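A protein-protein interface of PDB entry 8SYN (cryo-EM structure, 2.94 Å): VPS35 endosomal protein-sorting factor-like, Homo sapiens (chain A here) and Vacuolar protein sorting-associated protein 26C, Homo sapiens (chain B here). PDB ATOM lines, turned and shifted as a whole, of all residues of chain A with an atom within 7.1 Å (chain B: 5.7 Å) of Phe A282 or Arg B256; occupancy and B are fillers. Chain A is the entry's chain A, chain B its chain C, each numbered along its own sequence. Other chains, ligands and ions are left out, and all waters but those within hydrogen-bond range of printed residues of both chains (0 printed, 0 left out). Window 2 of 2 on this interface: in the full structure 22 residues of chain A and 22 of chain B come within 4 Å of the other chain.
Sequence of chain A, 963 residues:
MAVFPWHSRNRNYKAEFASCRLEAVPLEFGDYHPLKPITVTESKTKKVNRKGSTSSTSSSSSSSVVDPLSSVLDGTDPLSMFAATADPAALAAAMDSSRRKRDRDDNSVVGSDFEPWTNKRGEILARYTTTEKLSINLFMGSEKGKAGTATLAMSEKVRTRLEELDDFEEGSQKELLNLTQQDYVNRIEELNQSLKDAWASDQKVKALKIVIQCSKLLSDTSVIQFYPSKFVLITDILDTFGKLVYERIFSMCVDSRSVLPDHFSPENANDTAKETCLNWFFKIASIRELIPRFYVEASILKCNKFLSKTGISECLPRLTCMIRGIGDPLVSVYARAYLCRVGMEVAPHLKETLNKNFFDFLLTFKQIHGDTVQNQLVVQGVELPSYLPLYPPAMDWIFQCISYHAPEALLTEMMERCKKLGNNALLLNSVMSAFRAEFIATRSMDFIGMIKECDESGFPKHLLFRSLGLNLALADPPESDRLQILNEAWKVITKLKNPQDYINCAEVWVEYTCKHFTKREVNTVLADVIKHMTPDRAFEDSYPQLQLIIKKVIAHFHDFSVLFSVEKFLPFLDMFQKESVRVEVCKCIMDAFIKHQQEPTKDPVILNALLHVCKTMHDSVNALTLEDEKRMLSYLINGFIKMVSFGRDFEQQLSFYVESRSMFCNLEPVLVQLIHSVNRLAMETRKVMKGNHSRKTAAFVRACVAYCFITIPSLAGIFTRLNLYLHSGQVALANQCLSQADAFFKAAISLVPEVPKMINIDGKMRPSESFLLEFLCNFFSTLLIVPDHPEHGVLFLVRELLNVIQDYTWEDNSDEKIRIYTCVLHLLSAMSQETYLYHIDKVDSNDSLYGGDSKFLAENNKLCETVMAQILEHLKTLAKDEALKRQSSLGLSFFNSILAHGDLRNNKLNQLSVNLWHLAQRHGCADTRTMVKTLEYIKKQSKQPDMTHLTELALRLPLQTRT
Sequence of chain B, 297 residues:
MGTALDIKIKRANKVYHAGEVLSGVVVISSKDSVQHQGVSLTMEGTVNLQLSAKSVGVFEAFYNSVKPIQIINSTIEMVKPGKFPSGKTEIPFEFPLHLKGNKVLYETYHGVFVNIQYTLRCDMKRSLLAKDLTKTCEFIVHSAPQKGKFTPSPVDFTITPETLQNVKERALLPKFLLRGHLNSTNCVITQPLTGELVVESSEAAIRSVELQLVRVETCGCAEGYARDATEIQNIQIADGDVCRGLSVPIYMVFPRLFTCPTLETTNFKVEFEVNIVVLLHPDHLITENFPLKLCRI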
ATOM      1  N   GLU A 275       4.758  -9.666 -23.599  1.00  0.00           N
ATOM      2  CA  GLU A 275       5.816 -10.667 -23.569  1.00  0.00           C
ATOM      3  C   GLU A 275       7.191 -10.018 -23.508  1.00  0.00           C
ATOM      4  O   GLU A 275       8.060 -10.461 -22.748  1.00  0.00           O
ATOM      5  CB  GLU A 275       5.707 -11.590 -24.780  1.00  0.00           C
ATOM      6  CG  GLU A 275       6.750 -12.697 -24.806  1.00  0.00           C
ATOM      7  CD  GLU A 275       6.677 -13.608 -23.595  1.00  0.00           C
ATOM      8  OE1 GLU A 275       5.587 -13.731 -22.998  1.00  0.00           O
ATOM      9  OE2 GLU A 275       7.715 -14.204 -23.238  1.00  0.00           O
ATOM     10  N   THR A 276       7.409  -8.961 -24.294  1.00  0.00           N
ATOM     11  CA  THR A 276       8.690  -8.262 -24.243  1.00  0.00           C
ATOM     12  C   THR A 276       8.922  -7.631 -22.874  1.00  0.00           C
ATOM     13  O   THR A 276      10.033  -7.695 -22.329  1.00  0.00           O
ATOM     14  CB  THR A 276       8.756  -7.203 -25.339  1.00  0.00           C
ATOM     15  OG1 THR A 276       8.512  -7.817 -26.609  1.00  0.00           O
ATOM     16  CG2 THR A 276      10.123  -6.544 -25.359  1.00  0.00           C
ATOM     17  N   CYS A 277       7.881  -7.029 -22.295  1.00  0.00           N
ATOM     18  CA  CYS A 277       8.021  -6.412 -20.981  1.00  0.00           C
ATOM     19  C   CYS A 277       8.336  -7.451 -19.911  1.00  0.00           C
ATOM     20  O   CYS A 277       9.200  -7.227 -19.052  1.00  0.00           O
ATOM     21  CB  CYS A 277       6.747  -5.646 -20.633  1.00  0.00           C
ATOM     22  SG  CYS A 277       6.957  -4.378 -19.371  1.00  0.00           S
ATOM     23  N   LEU A 278       7.651  -8.595 -19.947  1.00  0.00           N
ATOM     24  CA  LEU A 278       7.927  -9.655 -18.985  1.00  0.00           C
ATOM     25  C   LEU A 278       9.330 -10.213 -19.169  1.00  0.00           C
ATOM     26  O   LEU A 278      10.009 -10.534 -18.187  1.00  0.00           O
ATOM     27  CB  LEU A 278       6.891 -10.769 -19.109  1.00  0.00           C
ATOM     28  CG  LEU A 278       5.645 -10.637 -18.239  1.00  0.00           C
ATOM     29  CD1 LEU A 278       4.544 -11.541 -18.756  1.00  0.00           C
ATOM     30  CD2 LEU A 278       5.972 -10.964 -16.792  1.00  0.00           C
ATOM     31  N   ASN A 279       9.780 -10.351 -20.418  1.00  0.00           N
ATOM     32  CA  ASN A 279      11.142 -10.814 -20.656  1.00  0.00           C
ATOM     33  C   ASN A 279      12.157  -9.850 -20.065  1.00  0.00           C
ATOM     34  O   ASN A 279      13.134 -10.275 -19.432  1.00  0.00           O
ATOM     35  CB  ASN A 279      11.382 -10.994 -22.152  1.00  0.00           C
ATOM     36  CG  ASN A 279      10.931 -12.344 -22.654  1.00  0.00           C
ATOM     37  OD1 ASN A 279      10.519 -13.203 -21.875  1.00  0.00           O
ATOM     38  ND2 ASN A 279      11.005 -12.544 -23.963  1.00  0.00           N
ATOM     39  N   TRP A 280      11.942  -8.546 -20.251  1.00  0.00           N
ATOM     40  CA  TRP A 280      12.860  -7.567 -19.680  1.00  0.00           C
ATOM     41  C   TRP A 280      12.857  -7.631 -18.160  1.00  0.00           C
ATOM     42  O   TRP A 280      13.921  -7.602 -17.524  1.00  0.00           O
ATOM     43  CB  TRP A 280      12.500  -6.163 -20.159  1.00  0.00           C
ATOM     44  CG  TRP A 280      13.163  -5.796 -21.443  1.00  0.00           C
ATOM     45  CD1 TRP A 280      12.554  -5.506 -22.624  1.00  0.00           C
ATOM     46  CD2 TRP A 280      14.571  -5.690 -21.681  1.00  0.00           C
ATOM     47  NE1 TRP A 280      13.493  -5.224 -23.584  1.00  0.00           N
ATOM     48  CE2 TRP A 280      14.739  -5.332 -23.027  1.00  0.00           C
ATOM     49  CE3 TRP A 280      15.704  -5.865 -20.884  1.00  0.00           C
ATOM     50  CZ2 TRP A 280      15.993  -5.141 -23.596  1.00  0.00           C
ATOM     51  CZ3 TRP A 280      16.946  -5.678 -21.449  1.00  0.00           C
ATOM     52  CH2 TRP A 280      17.081  -5.319 -22.791  1.00  0.00           C
ATOM     53  N   PHE A 281      11.673  -7.738 -17.558  1.00  0.00           N
ATOM     54  CA  PHE A 281      11.595  -7.782 -16.103  1.00  0.00           C
ATOM     55  C   PHE A 281      12.250  -9.039 -15.548  1.00  0.00           C
ATOM     56  O   PHE A 281      12.911  -8.987 -14.507  1.00  0.00           O
ATOM     57  CB  PHE A 281      10.143  -7.675 -15.648  1.00  0.00           C
ATOM     58  CG  PHE A 281       9.663  -6.263 -15.509  1.00  0.00           C
ATOM     59  CD1 PHE A 281      10.313  -5.383 -14.669  1.00  0.00           C
ATOM     60  CD2 PHE A 281       8.573  -5.815 -16.223  1.00  0.00           C
ATOM     61  CE1 PHE A 281       9.882  -4.085 -14.540  1.00  0.00           C
ATOM     62  CE2 PHE A 281       8.136  -4.516 -16.097  1.00  0.00           C
ATOM     63  CZ  PHE A 281       8.793  -3.650 -15.254  1.00  0.00           C
ATOM     64  N   PHE A 282      12.099 -10.175 -16.229  1.00  0.00           N
ATOM     65  CA  PHE A 282      12.735 -11.404 -15.765  1.00  0.00           C
ATOM     66  C   PHE A 282      14.250 -11.330 -15.909  1.00  0.00           C
ATOM     67  O   PHE A 282      14.994 -11.729 -15.002  1.00  0.00           O
ATOM     68  CB  PHE A 282      12.175 -12.601 -16.530  1.00  0.00           C
ATOM     69  CG  PHE A 282      11.011 -13.260 -15.852  1.00  0.00           C
ATOM     70  CD1 PHE A 282      11.214 -14.201 -14.861  1.00  0.00           C
ATOM     71  CD2 PHE A 282       9.715 -12.939 -16.207  1.00  0.00           C
ATOM     72  CE1 PHE A 282      10.147 -14.808 -14.238  1.00  0.00           C
ATOM     73  CE2 PHE A 282       8.645 -13.543 -15.586  1.00  0.00           C
ATOM     74  CZ  PHE A 282       8.861 -14.479 -14.601  1.00  0.00           C
ATOM     75  N   LYS A 283      14.729 -10.813 -17.046  1.00  0.00           N
ATOM     76  CA  LYS A 283      16.165 -10.637 -17.235  1.00  0.00           C
ATOM     77  C   LYS A 283      16.754  -9.755 -16.147  1.00  0.00           C
ATOM     78  O   LYS A 283      17.845 -10.029 -15.634  1.00  0.00           O
ATOM     79  CB  LYS A 283      16.443 -10.028 -18.608  1.00  0.00           C
ATOM     80  CG  LYS A 283      16.467 -11.017 -19.752  1.00  0.00           C
ATOM     81  CD  LYS A 283      16.998 -10.357 -21.014  1.00  0.00           C
ATOM     82  CE  LYS A 283      16.266 -10.848 -22.247  1.00  0.00           C
ATOM     83  NZ  LYS A 283      16.676 -10.099 -23.466  1.00  0.00           N
ATOM     84  N   ILE A 284      16.044  -8.689 -15.780  1.00  0.00           N
ATOM     85  CA  ILE A 284      16.549  -7.788 -14.749  1.00  0.00           C
ATOM     86  C   ILE A 284      16.452  -8.431 -13.369  1.00  0.00           C
ATOM     87  O   ILE A 284      17.332  -8.244 -12.522  1.00  0.00           O
ATOM     88  CB  ILE A 284      15.808  -6.446 -14.826  1.00  0.00           C
ATOM     89  CG1 ILE A 284      16.283  -5.698 -16.067  1.00  0.00           C
ATOM     90  CG2 ILE A 284      16.055  -5.621 -13.583  1.00  0.00           C
ATOM     91  CD1 ILE A 284      15.458  -4.524 -16.426  1.00  0.00           C
ATOM     92  N   ALA A 285      15.396  -9.204 -13.122  1.00  0.00           N
ATOM     93  CA  ALA A 285      15.275  -9.930 -11.867  1.00  0.00           C
ATOM     94  C   ALA A 285      16.309 -11.035 -11.726  1.00  0.00           C
ATOM     95  O   ALA A 285      16.498 -11.542 -10.617  1.00  0.00           O
ATOM     96  CB  ALA A 285      13.871 -10.523 -11.738  1.00  0.00           C
ATOM     97  N   SER A 286      16.970 -11.423 -12.811  1.00  0.00           N
ATOM     98  CA  SER A 286      18.007 -12.444 -12.751  1.00  0.00           C
ATOM     99  C   SER A 286      19.378 -11.894 -12.374  1.00  0.00           C
ATOM    100  O   SER A 286      20.338 -12.667 -12.309  1.00  0.00           O
ATOM    101  CB  SER A 286      18.107 -13.173 -14.092  1.00  0.00           C
ATOM    102  OG  SER A 286      19.323 -13.889 -14.189  1.00  0.00           O
ATOM    103  N   ILE A 287      19.497 -10.589 -12.126  1.00  0.00           N
ATOM    104  CA  ILE A 287      20.795  -9.999 -11.817  1.00  0.00           C
ATOM    105  C   ILE A 287      21.231 -10.400 -10.415  1.00  0.00           C
ATOM    106  O   ILE A 287      20.437 -10.390  -9.466  1.00  0.00           O
ATOM    107  CB  ILE A 287      20.740  -8.470 -11.968  1.00  0.00           C
ATOM    108  CG1 ILE A 287      20.318  -8.093 -13.383  1.00  0.00           C
ATOM    109  CG2 ILE A 287      22.089  -7.859 -11.659  1.00  0.00           C
ATOM    110  CD1 ILE A 287      20.114  -6.619 -13.578  1.00  0.00           C
ATOM    111  N   ASN B  13       3.721 -15.726 -26.134  1.00  0.00           N
ATOM    112  CA  ASN B  13       4.463 -16.374 -25.062  1.00  0.00           C
ATOM    113  C   ASN B  13       4.768 -17.841 -25.333  1.00  0.00           C
ATOM    114  O   ASN B  13       5.600 -18.419 -24.627  1.00  0.00           O
ATOM    115  CB  ASN B  13       3.715 -16.178 -23.731  1.00  0.00           C
ATOM    116  CG  ASN B  13       2.543 -17.137 -23.532  1.00  0.00           C
ATOM    117  OD1 ASN B  13       2.329 -18.080 -24.290  1.00  0.00           O
ATOM    118  ND2 ASN B  13       1.771 -16.883 -22.483  1.00  0.00           N
ATOM    119  N   GLU B 107       6.275 -30.692 -17.618  1.00  0.00           N
ATOM    120  CA  GLU B 107       6.614 -29.281 -17.701  1.00  0.00           C
ATOM    121  C   GLU B 107       7.922 -29.096 -18.458  1.00  0.00           C
ATOM    122  O   GLU B 107       8.857 -29.887 -18.312  1.00  0.00           O
ATOM    123  CB  GLU B 107       6.741 -28.697 -16.293  1.00  0.00           C
ATOM    124  CG  GLU B 107       7.270 -27.274 -16.236  1.00  0.00           C
ATOM    125  CD  GLU B 107       6.173 -26.244 -16.325  1.00  0.00           C
ATOM    126  OE1 GLU B 107       5.072 -26.598 -16.786  1.00  0.00           O
ATOM    127  OE2 GLU B 107       6.408 -25.082 -15.936  1.00  0.00           O
ATOM    128  N   THR B 108       7.983 -28.051 -19.280  1.00  0.00           N
ATOM    129  CA  THR B 108       9.238 -27.686 -19.922  1.00  0.00           C
ATOM    130  C   THR B 108      10.279 -27.345 -18.867  1.00  0.00           C
ATOM    131  O   THR B 108      10.012 -26.572 -17.942  1.00  0.00           O
ATOM    132  CB  THR B 108       9.029 -26.501 -20.860  1.00  0.00           C
ATOM    133  OG1 THR B 108       8.003 -26.814 -21.809  1.00  0.00           O
ATOM    134  CG2 THR B 108      10.310 -26.182 -21.601  1.00  0.00           C
ATOM    135  N   VAL B 253      12.804 -14.053  -7.636  1.00  0.00           N
ATOM    136  CA  VAL B 253      11.941 -14.397  -8.756  1.00  0.00           C
ATOM    137  C   VAL B 253      12.464 -15.674  -9.394  1.00  0.00           C
ATOM    138  O   VAL B 253      13.635 -15.750  -9.784  1.00  0.00           O
ATOM    139  CB  VAL B 253      11.881 -13.253  -9.779  1.00  0.00           C
ATOM    140  CG1 VAL B 253      11.081 -13.677 -10.991  1.00  0.00           C
ATOM    141  CG2 VAL B 253      11.273 -12.016  -9.147  1.00  0.00           C
ATOM    142  N   PHE B 254      11.605 -16.675  -9.498  1.00  0.00           N
ATOM    143  CA  PHE B 254      12.021 -17.957 -10.045  1.00  0.00           C
ATOM    144  C   PHE B 254      12.261 -17.833 -11.544  1.00  0.00           C
ATOM    145  O   PHE B 254      11.438 -17.241 -12.251  1.00  0.00           O
ATOM    146  CB  PHE B 254      10.970 -19.020  -9.758  1.00  0.00           C
ATOM    147  CG  PHE B 254      10.884 -19.404  -8.312  1.00  0.00           C
ATOM    148  CD1 PHE B 254      11.863 -20.181  -7.730  1.00  0.00           C
ATOM    149  CD2 PHE B 254       9.823 -18.988  -7.535  1.00  0.00           C
ATOM    150  CE1 PHE B 254      11.788 -20.532  -6.403  1.00  0.00           C
ATOM    151  CE2 PHE B 254       9.745 -19.341  -6.207  1.00  0.00           C
ATOM    152  CZ  PHE B 254      10.727 -20.116  -5.645  1.00  0.00           C
ATOM    153  N   PRO B 255      13.372 -18.355 -12.062  1.00  0.00           N
ATOM    154  CA  PRO B 255      13.615 -18.288 -13.505  1.00  0.00           C
ATOM    155  C   PRO B 255      12.555 -19.049 -14.287  1.00  0.00           C
ATOM    156  O   PRO B 255      11.960 -20.011 -13.799  1.00  0.00           O
ATOM    157  CB  PRO B 255      15.001 -18.921 -13.673  1.00  0.00           C
ATOM    158  CG  PRO B 255      15.344 -19.529 -12.376  1.00  0.00           C
ATOM    159  CD  PRO B 255      14.508 -18.915 -11.317  1.00  0.00           C
ATOM    160  N   ARG B 256      12.325 -18.595 -15.517  1.00  0.00           N
ATOM    161  CA  ARG B 256      11.210 -19.061 -16.331  1.00  0.00           C
ATOM    162  C   ARG B 256      11.283 -20.548 -16.643  1.00  0.00           C
ATOM    163  O   ARG B 256      10.430 -21.323 -16.198  1.00  0.00           O
ATOM    164  CB  ARG B 256      11.155 -18.269 -17.635  1.00  0.00           C
ATOM    165  CG  ARG B 256      10.946 -16.788 -17.443  1.00  0.00           C
ATOM    166  CD  ARG B 256       9.478 -16.439 -17.461  1.00  0.00           C
ATOM    167  NE  ARG B 256       8.937 -16.437 -18.814  1.00  0.00           N
ATOM    168  CZ  ARG B 256       9.209 -15.520 -19.733  1.00  0.00           C
ATOM    169  NH1 ARG B 256      10.019 -14.506 -19.480  1.00  0.00           N
ATOM    170  NH2 ARG B 256       8.651 -15.621 -20.935  1.00  0.00           N
ATOM    171  N   LEU B 257      12.294 -20.959 -17.403  1.00  0.00           N
ATOM    172  CA  LEU B 257      12.384 -22.333 -17.873  1.00  0.00           C
ATOM    173  C   LEU B 257      13.392 -23.168 -17.104  1.00  0.00           C
ATOM    174  O   LEU B 257      13.471 -24.378 -17.334  1.00  0.00           O
ATOM    175  CB  LEU B 257      12.733 -22.358 -19.363  1.00  0.00           C
ATOM    176  CG  LEU B 257      11.928 -21.406 -20.245  1.00  0.00           C
ATOM    177  CD1 LEU B 257      12.485 -21.373 -21.654  1.00  0.00           C
ATOM    178  CD2 LEU B 257      10.464 -21.808 -20.256  1.00  0.00           C
ATOM    179  N   PHE B 258      14.161 -22.563 -16.207  1.00  0.00           N
ATOM    180  CA  PHE B 258      15.094 -23.299 -15.370  1.00  0.00           C
ATOM    181  C   PHE B 258      14.447 -23.826 -14.099  1.00  0.00           C
ATOM    182  O   PHE B 258      15.103 -24.548 -13.341  1.00  0.00           O
ATOM    183  CB  PHE B 258      16.292 -22.415 -15.018  1.00  0.00           C
ATOM    184  CG  PHE B 258      16.951 -21.789 -16.211  1.00  0.00           C
ATOM    185  CD1 PHE B 258      17.622 -22.566 -17.133  1.00  0.00           C
ATOM    186  CD2 PHE B 258      16.890 -20.425 -16.414  1.00  0.00           C
ATOM    187  CE1 PHE B 258      18.225 -21.997 -18.230  1.00  0.00           C
ATOM    188  CE2 PHE B 258      17.492 -19.850 -17.511  1.00  0.00           C
ATOM    189  CZ  PHE B 258      18.159 -20.637 -18.419  1.00  0.00           C
ATOM    190  N   THR B 259      13.185 -23.487 -13.849  1.00  0.00           N
ATOM    191  CA  THR B 259      12.440 -23.985 -12.703  1.00  0.00           C
ATOM    192  C   THR B 259      11.109 -24.554 -13.167  1.00  0.00           C
ATOM    193  O   THR B 259      10.435 -23.970 -14.021  1.00  0.00           O
ATOM    194  CB  THR B 259      12.190 -22.890 -11.666  1.00  0.00           C
ATOM    195  OG1 THR B 259      11.502 -21.795 -12.279  1.00  0.00           O
ATOM    196  CG2 THR B 259      13.499 -22.403 -11.080  1.00  0.00           C
ATOM    197  N   CYS B 260      10.741 -25.691 -12.601  1.00  0.00           N
ATOM    198  CA  CYS B 260       9.491 -26.377 -12.872  1.00  0.00           C
ATOM    199  C   CYS B 260       8.882 -26.810 -11.549  1.00  0.00           C
ATOM    200  O   CYS B 260       9.578 -26.869 -10.531  1.00  0.00           O
ATOM    201  CB  CYS B 260       9.712 -27.602 -13.770  1.00  0.00           C
ATOM    202  SG  CYS B 260      10.832 -28.834 -13.091  1.00  0.00           S
ATOM    203  N   ARG B 296       2.083 -25.219  -9.100  1.00  0.00           N
ATOM    204  CA  ARG B 296       1.277 -24.287  -9.874  1.00  0.00           C
ATOM    205  C   ARG B 296      -0.168 -24.341  -9.405  1.00  0.00           C
ATOM    206  O   ARG B 296      -0.763 -25.421  -9.319  1.00  0.00           O
ATOM    207  CB  ARG B 296       1.342 -24.600 -11.368  1.00  0.00           C
ATOM    208  CG  ARG B 296       2.422 -23.847 -12.104  1.00  0.00           C
ATOM    209  CD  ARG B 296       2.301 -24.017 -13.600  1.00  0.00           C
ATOM    210  NE  ARG B 296       3.576 -23.769 -14.258  1.00  0.00           N
ATOM    211  CZ  ARG B 296       4.069 -22.564 -14.502  1.00  0.00           C
ATOM    212  NH1 ARG B 296       3.405 -21.466 -14.182  1.00  0.00           N
ATOM    213  NH2 ARG B 296       5.263 -22.455 -15.077  1.00  0.00           N
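OE2 of Glu A275 is in salt-bridge range of NH2 of Arg B256.
The side-chain amide oxygen (OD1) of Asn A279 is in hydrogen-bond range of the guanidinium group (NH1) of Arg B256 (2.8 Å).
Among the printed residues, merely in contact across the chains: Glu A275 with Asn B13, Phe A282 with Phe B254, Phe A282 with Arg B256, Phe A282 with Val B253 and Ala A285 with Val B253.
Of the 13 printed residues of chain A, 4 touch a printed residue of chain B.
Of the 12 printed residues of chain B, 4 touch a printed residue of chain A.
Printed residues of chain B that touch a printed residue of chain A: Asn B13, Val B253, Phe B254 and Arg B256.
Hydrophobic or aromatic side chains of chain B within 4 Å of the printed part of chain A: Val B253.
Among the printed residues, 7 pairs touch across the chains.
The side-chain carboxylate (OE2) of Glu A275 lies close to the side-chain amide oxygen (OD1) of Asn A279 (3.3 Å).
Phe A282 touches just these residues of chain B: Val B253 (3.6 Å), Phe B254 (3.4 Å) and Arg B256 (3.5 Å).
Of the printed residues of chain A, Arg B256 touches Glu A275, Asn A279 and Phe A282.
Of the printed residues of chain B, Ala A285 touches Val B253.
Printed residues of chain B within 4 Å of Asn A279: Arg B256 (2.8 Å).
Printed residues of chain B within 4 Å of Glu A275: Asn B13 and Arg B256.
Printed residues of chain A within 4 Å of Val B253: Phe A282 and Ala A285.
The nearest residue of chain B that does not touch Phe A282 is Pro B255 (4.9 Å).
The nearest residue of chain A that does not touch Arg B256 is Leu A278 (4.2 Å).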
